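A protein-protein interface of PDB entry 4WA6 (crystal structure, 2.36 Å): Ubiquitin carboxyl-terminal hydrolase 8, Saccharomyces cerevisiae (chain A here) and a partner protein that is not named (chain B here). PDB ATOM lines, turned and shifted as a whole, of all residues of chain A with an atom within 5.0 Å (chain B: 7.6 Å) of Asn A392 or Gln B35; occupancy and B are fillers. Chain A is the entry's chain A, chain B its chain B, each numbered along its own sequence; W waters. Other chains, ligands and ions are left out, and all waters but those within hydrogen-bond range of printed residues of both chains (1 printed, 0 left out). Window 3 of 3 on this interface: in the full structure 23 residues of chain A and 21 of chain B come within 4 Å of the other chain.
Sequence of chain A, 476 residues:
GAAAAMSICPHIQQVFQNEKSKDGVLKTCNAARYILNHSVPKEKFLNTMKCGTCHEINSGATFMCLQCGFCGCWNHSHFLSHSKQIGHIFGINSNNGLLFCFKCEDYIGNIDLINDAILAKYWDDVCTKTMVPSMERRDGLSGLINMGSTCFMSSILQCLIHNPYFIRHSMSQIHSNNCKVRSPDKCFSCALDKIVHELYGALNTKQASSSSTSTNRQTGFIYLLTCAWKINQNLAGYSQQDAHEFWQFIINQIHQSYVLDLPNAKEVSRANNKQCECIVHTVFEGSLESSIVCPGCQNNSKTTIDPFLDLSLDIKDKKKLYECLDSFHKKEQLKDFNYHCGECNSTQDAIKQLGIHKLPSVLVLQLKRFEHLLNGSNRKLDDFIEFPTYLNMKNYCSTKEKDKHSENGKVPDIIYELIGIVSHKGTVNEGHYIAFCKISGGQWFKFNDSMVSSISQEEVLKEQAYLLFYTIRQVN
ND2 of Asn A392 sits at hydrogen-bond distance from OE1 of Gln B35 (3.1 Å). The side-chain carboxylate of Asp B40 sits close to the side-chain hydroxyl of Tyr A390, 3.2 Å away.
Among the printed residues, pairs that only touch across the chains: Tyr A390 with Leu B34, Ile A415 with Ala B31, Ile A415 with Gln B35, Ile A415 with Leu B34 and Asp A413 with Ala B31.
Asn A392 touches just one residue of chain B: Gln B35. Printed residues of chain A within 4 Å of Gln B35: Asn A392 and Ile A415. Of the printed residues of chain B, Asp A413 touches Ala B31. Printed residues of chain A within 4 Å of Ala B31: Asp A413 (3.98 Å) and Ile A415 (3.5 Å). Printed residues of chain A within 4 Å of Leu B34: Tyr A390 and Ile A415. Of the printed residues of chain B, Ile A415 touches Ala B31 (3.5 Å), Leu B34 (3.8 Å) and Gln B35 (3.6 Å). Of the printed residues of chain A, Asp B40 touches Tyr A390 (2.9 Å). Pro A412 touches none of the printed residues of chain B. Met A393 touches none of the printed residues of chain B. The nearest printed residue of chain A that does not touch Leu B34 is Leu A391 (7.4 Å).
Of the 13 printed residues of chain B, 4 touch a printed residue of chain A. Hydrophobic or aromatic side chains of chain B that line the printed part of chain A: Ala B31 and Leu B34. Printed residues of chain A that touch a printed residue of chain B: Tyr A390, Asn A392, Asp A413 and Ile A415.
OD1 of Asn A392 lies within hydrogen-bond range of N of Lys A394, 3.1 Å away. ND2 of Asn A392 sits at hydrogen-bond distance from OD1 of Asp A413, at 3.3 Å. The side-chain hydroxyl (OH) of Tyr A322 sits at hydrogen-bond distance from the backbone NH (N) of Asn A392 (2.8 Å). O of Ala B31 lies within hydrogen-bond range of NE2 of Gln B35 (3.1 Å). The side-chain amide oxygen (OD1) of Asn A392 lies within hydrogen-bond range of the backbone NH (N) of Ile A414 (3.4 Å). The side-chain amino group (NZ) of Lys A394 is in salt-bridge range of the side-chain carboxylate (OD1) of Asp A413, at 2.7 Å.
Water W1 lies within hydrogen-bond range of the side-chain carboxylate (OD1) of Asp A413 (2.9 Å), the side-chain amide nitrogen (NE2) of Gln B35 (3.0 Å) and the side-chain amide nitrogen (ND2) of Asn A392 (3.4 Å).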
ATOM      1  N   TYR A 322      20.980  36.344  11.341  1.00  0.00           N
ATOM      2  CA  TYR A 322      19.723  36.529  12.087  1.00  0.00           C
ATOM      3  C   TYR A 322      19.507  38.003  12.531  1.00  0.00           C
ATOM      4  O   TYR A 322      18.366  38.486  12.551  1.00  0.00           O
ATOM      5  CB  TYR A 322      19.637  35.568  13.283  1.00  0.00           C
ATOM      6  CG  TYR A 322      19.222  34.163  12.936  1.00  0.00           C
ATOM      7  CD1 TYR A 322      18.010  33.908  12.288  1.00  0.00           C
ATOM      8  CD2 TYR A 322      20.017  33.060  13.284  1.00  0.00           C
ATOM      9  CE1 TYR A 322      17.590  32.618  12.004  1.00  0.00           C
ATOM     10  CE2 TYR A 322      19.620  31.758  12.963  1.00  0.00           C
ATOM     11  CZ  TYR A 322      18.396  31.546  12.338  1.00  0.00           C
ATOM     12  OH  TYR A 322      17.974  30.256  12.020  1.00  0.00           O
ATOM     13  N   TYR A 390      21.545  25.803   8.655  1.00  0.00           N
ATOM     14  CA  TYR A 390      20.107  25.582   8.721  1.00  0.00           C
ATOM     15  C   TYR A 390      19.540  26.868   9.200  1.00  0.00           C
ATOM     16  O   TYR A 390      20.036  27.407  10.153  1.00  0.00           O
ATOM     17  CB  TYR A 390      19.785  24.407   9.640  1.00  0.00           C
ATOM     18  CG  TYR A 390      20.159  23.130   8.957  1.00  0.00           C
ATOM     19  CD1 TYR A 390      19.344  22.595   7.997  1.00  0.00           C
ATOM     20  CD2 TYR A 390      21.370  22.507   9.202  1.00  0.00           C
ATOM     21  CE1 TYR A 390      19.716  21.465   7.293  1.00  0.00           C
ATOM     22  CE2 TYR A 390      21.734  21.382   8.516  1.00  0.00           C
ATOM     23  CZ  TYR A 390      20.917  20.874   7.553  1.00  0.00           C
ATOM     24  OH  TYR A 390      21.262  19.731   6.856  1.00  0.00           O
ATOM     25  N   LEU A 391      18.595  27.426   8.464  1.00  0.00           N
ATOM     26  CA  LEU A 391      18.047  28.727   8.755  1.00  0.00           C
ATOM     27  C   LEU A 391      16.565  28.585   9.063  1.00  0.00           C
ATOM     28  O   LEU A 391      15.806  28.031   8.279  1.00  0.00           O
ATOM     29  CB  LEU A 391      18.164  29.601   7.512  1.00  0.00           C
ATOM     30  CG  LEU A 391      17.426  30.956   7.569  1.00  0.00           C
ATOM     31  CD1 LEU A 391      18.075  31.910   8.561  1.00  0.00           C
ATOM     32  CD2 LEU A 391      17.399  31.586   6.201  1.00  0.00           C
ATOM     33  N   ASN A 392      16.135  29.139  10.171  1.00  0.00           N
ATOM     34  CA  ASN A 392      14.757  29.058  10.538  1.00  0.00           C
ATOM     35  C   ASN A 392      14.008  30.393  10.264  1.00  0.00           C
ATOM     36  O   ASN A 392      14.289  31.424  10.901  1.00  0.00           O
ATOM     37  CB  ASN A 392      14.708  28.750  12.021  1.00  0.00           C
ATOM     38  CG  ASN A 392      13.343  28.325  12.484  1.00  0.00           C
ATOM     39  OD1 ASN A 392      12.312  28.768  11.969  1.00  0.00           O
ATOM     40  ND2 ASN A 392      13.327  27.455  13.468  1.00  0.00           N
ATOM     41  N   MET A 393      13.022  30.370   9.384  1.00  0.00           N
ATOM     42  CA  MET A 393      12.334  31.612   9.074  1.00  0.00           C
ATOM     43  C   MET A 393      11.130  31.971   9.916  1.00  0.00           C
ATOM     44  O   MET A 393      10.463  32.922   9.597  1.00  0.00           O
ATOM     45  CB  MET A 393      11.995  31.663   7.593  1.00  0.00           C
ATOM     46  CG  MET A 393      13.286  31.707   6.802  1.00  0.00           C
ATOM     47  SD  MET A 393      14.238  33.232   7.064  1.00  0.00           S
ATOM     48  CE  MET A 393      13.117  34.294   6.173  1.00  0.00           C
ATOM     49  N   LYS A 394      10.870  31.283  11.021  1.00  0.00           N
ATOM     50  CA  LYS A 394       9.587  31.474  11.668  1.00  0.00           C
ATOM     51  C   LYS A 394       9.370  32.879  12.263  1.00  0.00           C
ATOM     52  O   LYS A 394       8.260  33.318  12.303  1.00  0.00           O
ATOM     53  CB  LYS A 394       9.302  30.395  12.707  1.00  0.00           C
ATOM     54  CG  LYS A 394      10.070  30.535  13.990  1.00  0.00           C
ATOM     55  CD  LYS A 394       9.667  29.415  14.929  1.00  0.00           C
ATOM     56  CE  LYS A 394      10.463  29.425  16.216  1.00  0.00           C
ATOM     57  NZ  LYS A 394      10.060  28.228  16.997  1.00  0.00           N
ATOM     58  N   ASN A 395      10.419  33.582  12.685  1.00  0.00           N
ATOM     59  CA  ASN A 395      10.257  34.920  13.293  1.00  0.00           C
ATOM     60  C   ASN A 395      10.137  36.041  12.285  1.00  0.00           C
ATOM     61  O   ASN A 395      10.201  37.209  12.639  1.00  0.00           O
ATOM     62  CB  ASN A 395      11.456  35.228  14.172  1.00  0.00           C
ATOM     63  CG  ASN A 395      11.538  34.310  15.348  1.00  0.00           C
ATOM     64  OD1 ASN A 395      10.575  33.673  15.687  1.00  0.00           O
ATOM     65  ND2 ASN A 395      12.684  34.223  15.954  1.00  0.00           N
ATOM     66  N   TYR A 396      10.065  35.688  11.005  1.00  0.00           N
ATOM     67  CA  TYR A 396      10.061  36.691   9.971  1.00  0.00           C
ATOM     68  C   TYR A 396       8.789  36.594   9.172  1.00  0.00           C
ATOM     69  O   TYR A 396       8.571  37.399   8.289  1.00  0.00           O
ATOM     70  CB  TYR A 396      11.345  36.548   9.138  1.00  0.00           C
ATOM     71  CG  TYR A 396      12.531  36.531  10.068  1.00  0.00           C
ATOM     72  CD1 TYR A 396      12.856  37.647  10.781  1.00  0.00           C
ATOM     73  CD2 TYR A 396      13.295  35.377  10.268  1.00  0.00           C
ATOM     74  CE1 TYR A 396      13.893  37.651  11.698  1.00  0.00           C
ATOM     75  CE2 TYR A 396      14.362  35.373  11.145  1.00  0.00           C
ATOM     76  CZ  TYR A 396      14.642  36.519  11.875  1.00  0.00           C
ATOM     77  OH  TYR A 396      15.691  36.577  12.766  1.00  0.00           O
ATOM     78  N   PRO A 412       5.050  28.144  13.100  1.00  0.00           N
ATOM     79  CA  PRO A 412       5.886  26.979  13.351  1.00  0.00           C
ATOM     80  C   PRO A 412       7.265  27.033  12.693  1.00  0.00           C
ATOM     81  O   PRO A 412       7.505  27.837  11.783  1.00  0.00           O
ATOM     82  CB  PRO A 412       5.099  25.856  12.672  1.00  0.00           C
ATOM     83  CG  PRO A 412       4.413  26.534  11.531  1.00  0.00           C
ATOM     84  CD  PRO A 412       4.036  27.883  12.070  1.00  0.00           C
ATOM     85  N   ASP A 413       8.150  26.148  13.140  1.00  0.00           N
ATOM     86  CA  ASP A 413       9.462  26.115  12.638  1.00  0.00           C
ATOM     87  C   ASP A 413       9.359  25.915  11.111  1.00  0.00           C
ATOM     88  O   ASP A 413       8.598  25.082  10.615  1.00  0.00           O
ATOM     89  CB  ASP A 413      10.255  24.985  13.276  1.00  0.00           C
ATOM     90  CG  ASP A 413      10.601  25.240  14.752  1.00  0.00           C
ATOM     91  OD1 ASP A 413      10.769  26.386  15.203  1.00  0.00           O
ATOM     92  OD2 ASP A 413      10.738  24.251  15.480  1.00  0.00           O
ATOM     93  N   ILE A 414      10.096  26.734  10.380  1.00  0.00           N
ATOM     94  CA  ILE A 414      10.197  26.586   8.970  1.00  0.00           C
ATOM     95  C   ILE A 414      11.655  26.678   8.631  1.00  0.00           C
ATOM     96  O   ILE A 414      12.216  27.769   8.605  1.00  0.00           O
ATOM     97  CB  ILE A 414       9.445  27.708   8.276  1.00  0.00           C
ATOM     98  CG1 ILE A 414       7.960  27.542   8.502  1.00  0.00           C
ATOM     99  CG2 ILE A 414       9.700  27.666   6.778  1.00  0.00           C
ATOM    100  CD1 ILE A 414       7.209  28.807   8.226  1.00  0.00           C
ATOM    101  N   ILE A 415      12.249  25.528   8.327  1.00  0.00           N
ATOM    102  CA  ILE A 415      13.684  25.389   8.219  1.00  0.00           C
ATOM    103  C   ILE A 415      14.144  25.135   6.802  1.00  0.00           C
ATOM    104  O   ILE A 415      13.618  24.269   6.082  1.00  0.00           O
ATOM    105  CB  ILE A 415      14.168  24.256   9.171  1.00  0.00           C
ATOM    106  CG1 ILE A 415      13.702  24.568  10.591  1.00  0.00           C
ATOM    107  CG2 ILE A 415      15.678  24.151   9.191  1.00  0.00           C
ATOM    108  CD1 ILE A 415      13.867  23.439  11.547  1.00  0.00           C
ATOM    109  N   GLU B  28       9.029  17.925  16.164  1.00  0.00           N
ATOM    110  CA  GLU B  28       9.810  18.810  16.990  1.00  0.00           C
ATOM    111  C   GLU B  28      11.227  18.260  17.056  1.00  0.00           C
ATOM    112  O   GLU B  28      12.202  18.994  16.996  1.00  0.00           O
ATOM    113  CB  GLU B  28       9.165  18.847  18.359  1.00  0.00           C
ATOM    114  CG  GLU B  28       9.988  19.420  19.469  1.00  0.00           C
ATOM    115  CD  GLU B  28      10.001  20.924  19.458  1.00  0.00           C
ATOM    116  OE1 GLU B  28       9.853  21.534  18.375  1.00  0.00           O
ATOM    117  OE2 GLU B  28      10.195  21.490  20.547  1.00  0.00           O
ATOM    118  N   LEU B  29      11.318  16.956  17.217  1.00  0.00           N
ATOM    119  CA  LEU B  29      12.578  16.302  17.407  1.00  0.00           C
ATOM    120  C   LEU B  29      13.455  16.523  16.202  1.00  0.00           C
ATOM    121  O   LEU B  29      14.638  16.851  16.343  1.00  0.00           O
ATOM    122  CB  LEU B  29      12.362  14.783  17.620  1.00  0.00           C
ATOM    123  CG  LEU B  29      13.619  13.977  17.659  1.00  0.00           C
ATOM    124  CD1 LEU B  29      14.604  14.421  18.733  1.00  0.00           C
ATOM    125  CD2 LEU B  29      13.280  12.519  17.856  1.00  0.00           C
ATOM    126  N   LYS B  30      12.910  16.292  15.009  1.00  0.00           N
ATOM    127  CA  LYS B  30      13.729  16.399  13.806  1.00  0.00           C
ATOM    128  C   LYS B  30      14.164  17.802  13.569  1.00  0.00           C
ATOM    129  O   LYS B  30      15.265  18.007  13.077  1.00  0.00           O
ATOM    130  CB  LYS B  30      12.989  15.927  12.568  1.00  0.00           C
ATOM    131  CG  LYS B  30      12.657  14.470  12.683  1.00  0.00           C
ATOM    132  CD  LYS B  30      11.626  14.037  11.687  1.00  0.00           C
ATOM    133  CE  LYS B  30      11.449  12.536  11.797  1.00  0.00           C
ATOM    134  NZ  LYS B  30      10.670  12.125  10.615  1.00  0.00           N
ATOM    135  N   ALA B  31      13.301  18.775  13.881  1.00  0.00           N
ATOM    136  CA  ALA B  31      13.693  20.159  13.658  1.00  0.00           C
ATOM    137  C   ALA B  31      14.857  20.539  14.570  1.00  0.00           C
ATOM    138  O   ALA B  31      15.764  21.275  14.162  1.00  0.00           O
ATOM    139  CB  ALA B  31      12.538  21.107  13.840  1.00  0.00           C
ATOM    140  N   ARG B  32      14.834  20.026  15.785  1.00  0.00           N
ATOM    141  CA  ARG B  32      15.916  20.246  16.711  1.00  0.00           C
ATOM    142  C   ARG B  32      17.162  19.546  16.266  1.00  0.00           C
ATOM    143  O   ARG B  32      18.216  20.118  16.316  1.00  0.00           O
ATOM    144  CB  ARG B  32      15.535  19.779  18.121  1.00  0.00           C
ATOM    145  CG  ARG B  32      14.555  20.727  18.764  1.00  0.00           C
ATOM    146  CD  ARG B  32      14.057  20.174  20.087  1.00  0.00           C
ATOM    147  NE  ARG B  32      13.253  21.186  20.750  1.00  0.00           N
ATOM    148  CZ  ARG B  32      13.770  22.222  21.422  1.00  0.00           C
ATOM    149  NH1 ARG B  32      15.092  22.370  21.566  1.00  0.00           N
ATOM    150  NH2 ARG B  32      12.964  23.109  21.969  1.00  0.00           N
ATOM    151  N   LEU B  33      17.048  18.311  15.817  1.00  0.00           N
ATOM    152  CA  LEU B  33      18.235  17.585  15.380  1.00  0.00           C
ATOM    153  C   LEU B  33      18.842  18.236  14.142  1.00  0.00           C
ATOM    154  O   LEU B  33      20.034  18.349  14.027  1.00  0.00           O
ATOM    155  CB  LEU B  33      17.891  16.128  15.102  1.00  0.00           C
ATOM    156  CG  LEU B  33      17.482  15.399  16.375  1.00  0.00           C
ATOM    157  CD1 LEU B  33      17.036  13.996  16.068  1.00  0.00           C
ATOM    158  CD2 LEU B  33      18.609  15.355  17.387  1.00  0.00           C
ATOM    159  N   LEU B  34      18.019  18.696  13.234  1.00  0.00           N
ATOM    160  CA  LEU B  34      18.505  19.367  12.058  1.00  0.00           C
ATOM    161  C   LEU B  34      19.247  20.608  12.492  1.00  0.00           C
ATOM    162  O   LEU B  34      20.438  20.799  12.175  1.00  0.00           O
ATOM    163  CB  LEU B  34      17.318  19.730  11.169  1.00  0.00           C
ATOM    164  CG  LEU B  34      17.588  20.206   9.759  1.00  0.00           C
ATOM    165  CD1 LEU B  34      18.501  19.204   9.056  1.00  0.00           C
ATOM    166  CD2 LEU B  34      16.277  20.400   9.013  1.00  0.00           C
ATOM    167  N   GLN B  35      18.559  21.445  13.267  1.00  0.00           N
ATOM    168  CA  GLN B  35      19.155  22.741  13.600  1.00  0.00           C
ATOM    169  C   GLN B  35      20.453  22.633  14.393  1.00  0.00           C
ATOM    170  O   GLN B  35      21.387  23.396  14.121  1.00  0.00           O
ATOM    171  CB  GLN B  35      18.177  23.634  14.321  1.00  0.00           C
ATOM    172  CG  GLN B  35      17.110  24.123  13.377  1.00  0.00           C
ATOM    173  CD  GLN B  35      16.081  24.931  14.068  1.00  0.00           C
ATOM    174  OE1 GLN B  35      16.100  26.118  13.956  1.00  0.00           O
ATOM    175  NE2 GLN B  35      15.180  24.287  14.799  1.00  0.00           N
ATOM    176  N   GLU B  36      20.540  21.681  15.329  1.00  0.00           N
ATOM    177  CA  GLU B  36      21.771  21.539  16.112  1.00  0.00           C
ATOM    178  C   GLU B  36      22.961  20.839  15.358  1.00  0.00           C
ATOM    179  O   GLU B  36      23.985  20.579  15.960  1.00  0.00           O
ATOM    180  CB  GLU B  36      21.488  20.879  17.478  1.00  0.00           C
ATOM    181  CG  GLU B  36      21.414  19.353  17.454  1.00  0.00           C
ATOM    182  CD  GLU B  36      20.836  18.785  18.765  1.00  0.00           C
ATOM    183  OE1 GLU B  36      19.884  19.445  19.267  1.00  0.00           O
ATOM    184  OE2 GLU B  36      21.333  17.700  19.281  1.00  0.00           O
ATOM    185  N   GLY B  37      22.846  20.527  14.077  1.00  0.00           N
ATOM    186  CA  GLY B  37      23.994  19.943  13.339  1.00  0.00           C
ATOM    187  C   GLY B  37      24.083  18.420  13.441  1.00  0.00           C
ATOM    188  O   GLY B  37      24.934  17.799  12.790  1.00  0.00           O
ATOM    189  N   TRP B  38      23.162  17.819  14.208  1.00  0.00           N
ATOM    190  CA  TRP B  38      23.191  16.409  14.538  1.00  0.00           C
ATOM    191  C   TRP B  38      23.027  15.566  13.311  1.00  0.00           C
ATOM    192  O   TRP B  38      23.808  14.609  13.125  1.00  0.00           O
ATOM    193  CB  TRP B  38      22.112  16.051  15.585  1.00  0.00           C
ATOM    194  CG  TRP B  38      22.024  14.636  15.963  1.00  0.00           C
ATOM    195  CD1 TRP B  38      22.665  14.009  17.020  1.00  0.00           C
ATOM    196  CD2 TRP B  38      21.265  13.611  15.297  1.00  0.00           C
ATOM    197  NE1 TRP B  38      22.310  12.669  17.061  1.00  0.00           N
ATOM    198  CE2 TRP B  38      21.472  12.405  16.004  1.00  0.00           C
ATOM    199  CE3 TRP B  38      20.447  13.596  14.174  1.00  0.00           C
ATOM    200  CZ2 TRP B  38      20.862  11.224  15.629  1.00  0.00           C
ATOM    201  CZ3 TRP B  38      19.846  12.425  13.801  1.00  0.00           C
ATOM    202  CH2 TRP B  38      20.045  11.260  14.517  1.00  0.00           C
ATOM    203  N   VAL B  39      22.035  15.878  12.466  1.00  0.00           N
ATOM    204  CA  VAL B  39      21.893  15.050  11.243  1.00  0.00           C
ATOM    205  C   VAL B  39      23.189  15.017  10.447  1.00  0.00           C
ATOM    206  O   VAL B  39      23.599  13.978   9.967  1.00  0.00           O
ATOM    207  CB  VAL B  39      20.763  15.465  10.281  1.00  0.00           C
ATOM    208  CG1 VAL B  39      20.746  14.501   9.093  1.00  0.00           C
ATOM    209  CG2 VAL B  39      19.415  15.458  11.006  1.00  0.00           C
ATOM    210  N   ASP B  40      23.855  16.140  10.344  1.00  0.00           N
ATOM    211  CA  ASP B  40      25.062  16.196   9.549  1.00  0.00           C
ATOM    212  C   ASP B  40      26.200  15.418  10.226  1.00  0.00           C
ATOM    213  O   ASP B  40      26.913  14.659   9.568  1.00  0.00           O
ATOM    214  CB  ASP B  40      25.413  17.636   9.259  1.00  0.00           C
ATOM    215  CG  ASP B  40      24.368  18.296   8.384  1.00  0.00           C
ATOM    216  OD1 ASP B  40      24.091  17.742   7.304  1.00  0.00           O
ATOM    217  OD2 ASP B  40      23.796  19.347   8.758  1.00  0.00           O
HETATM  218  O   HOH W   1      13.269  25.815  16.478  1.00  0.00           O
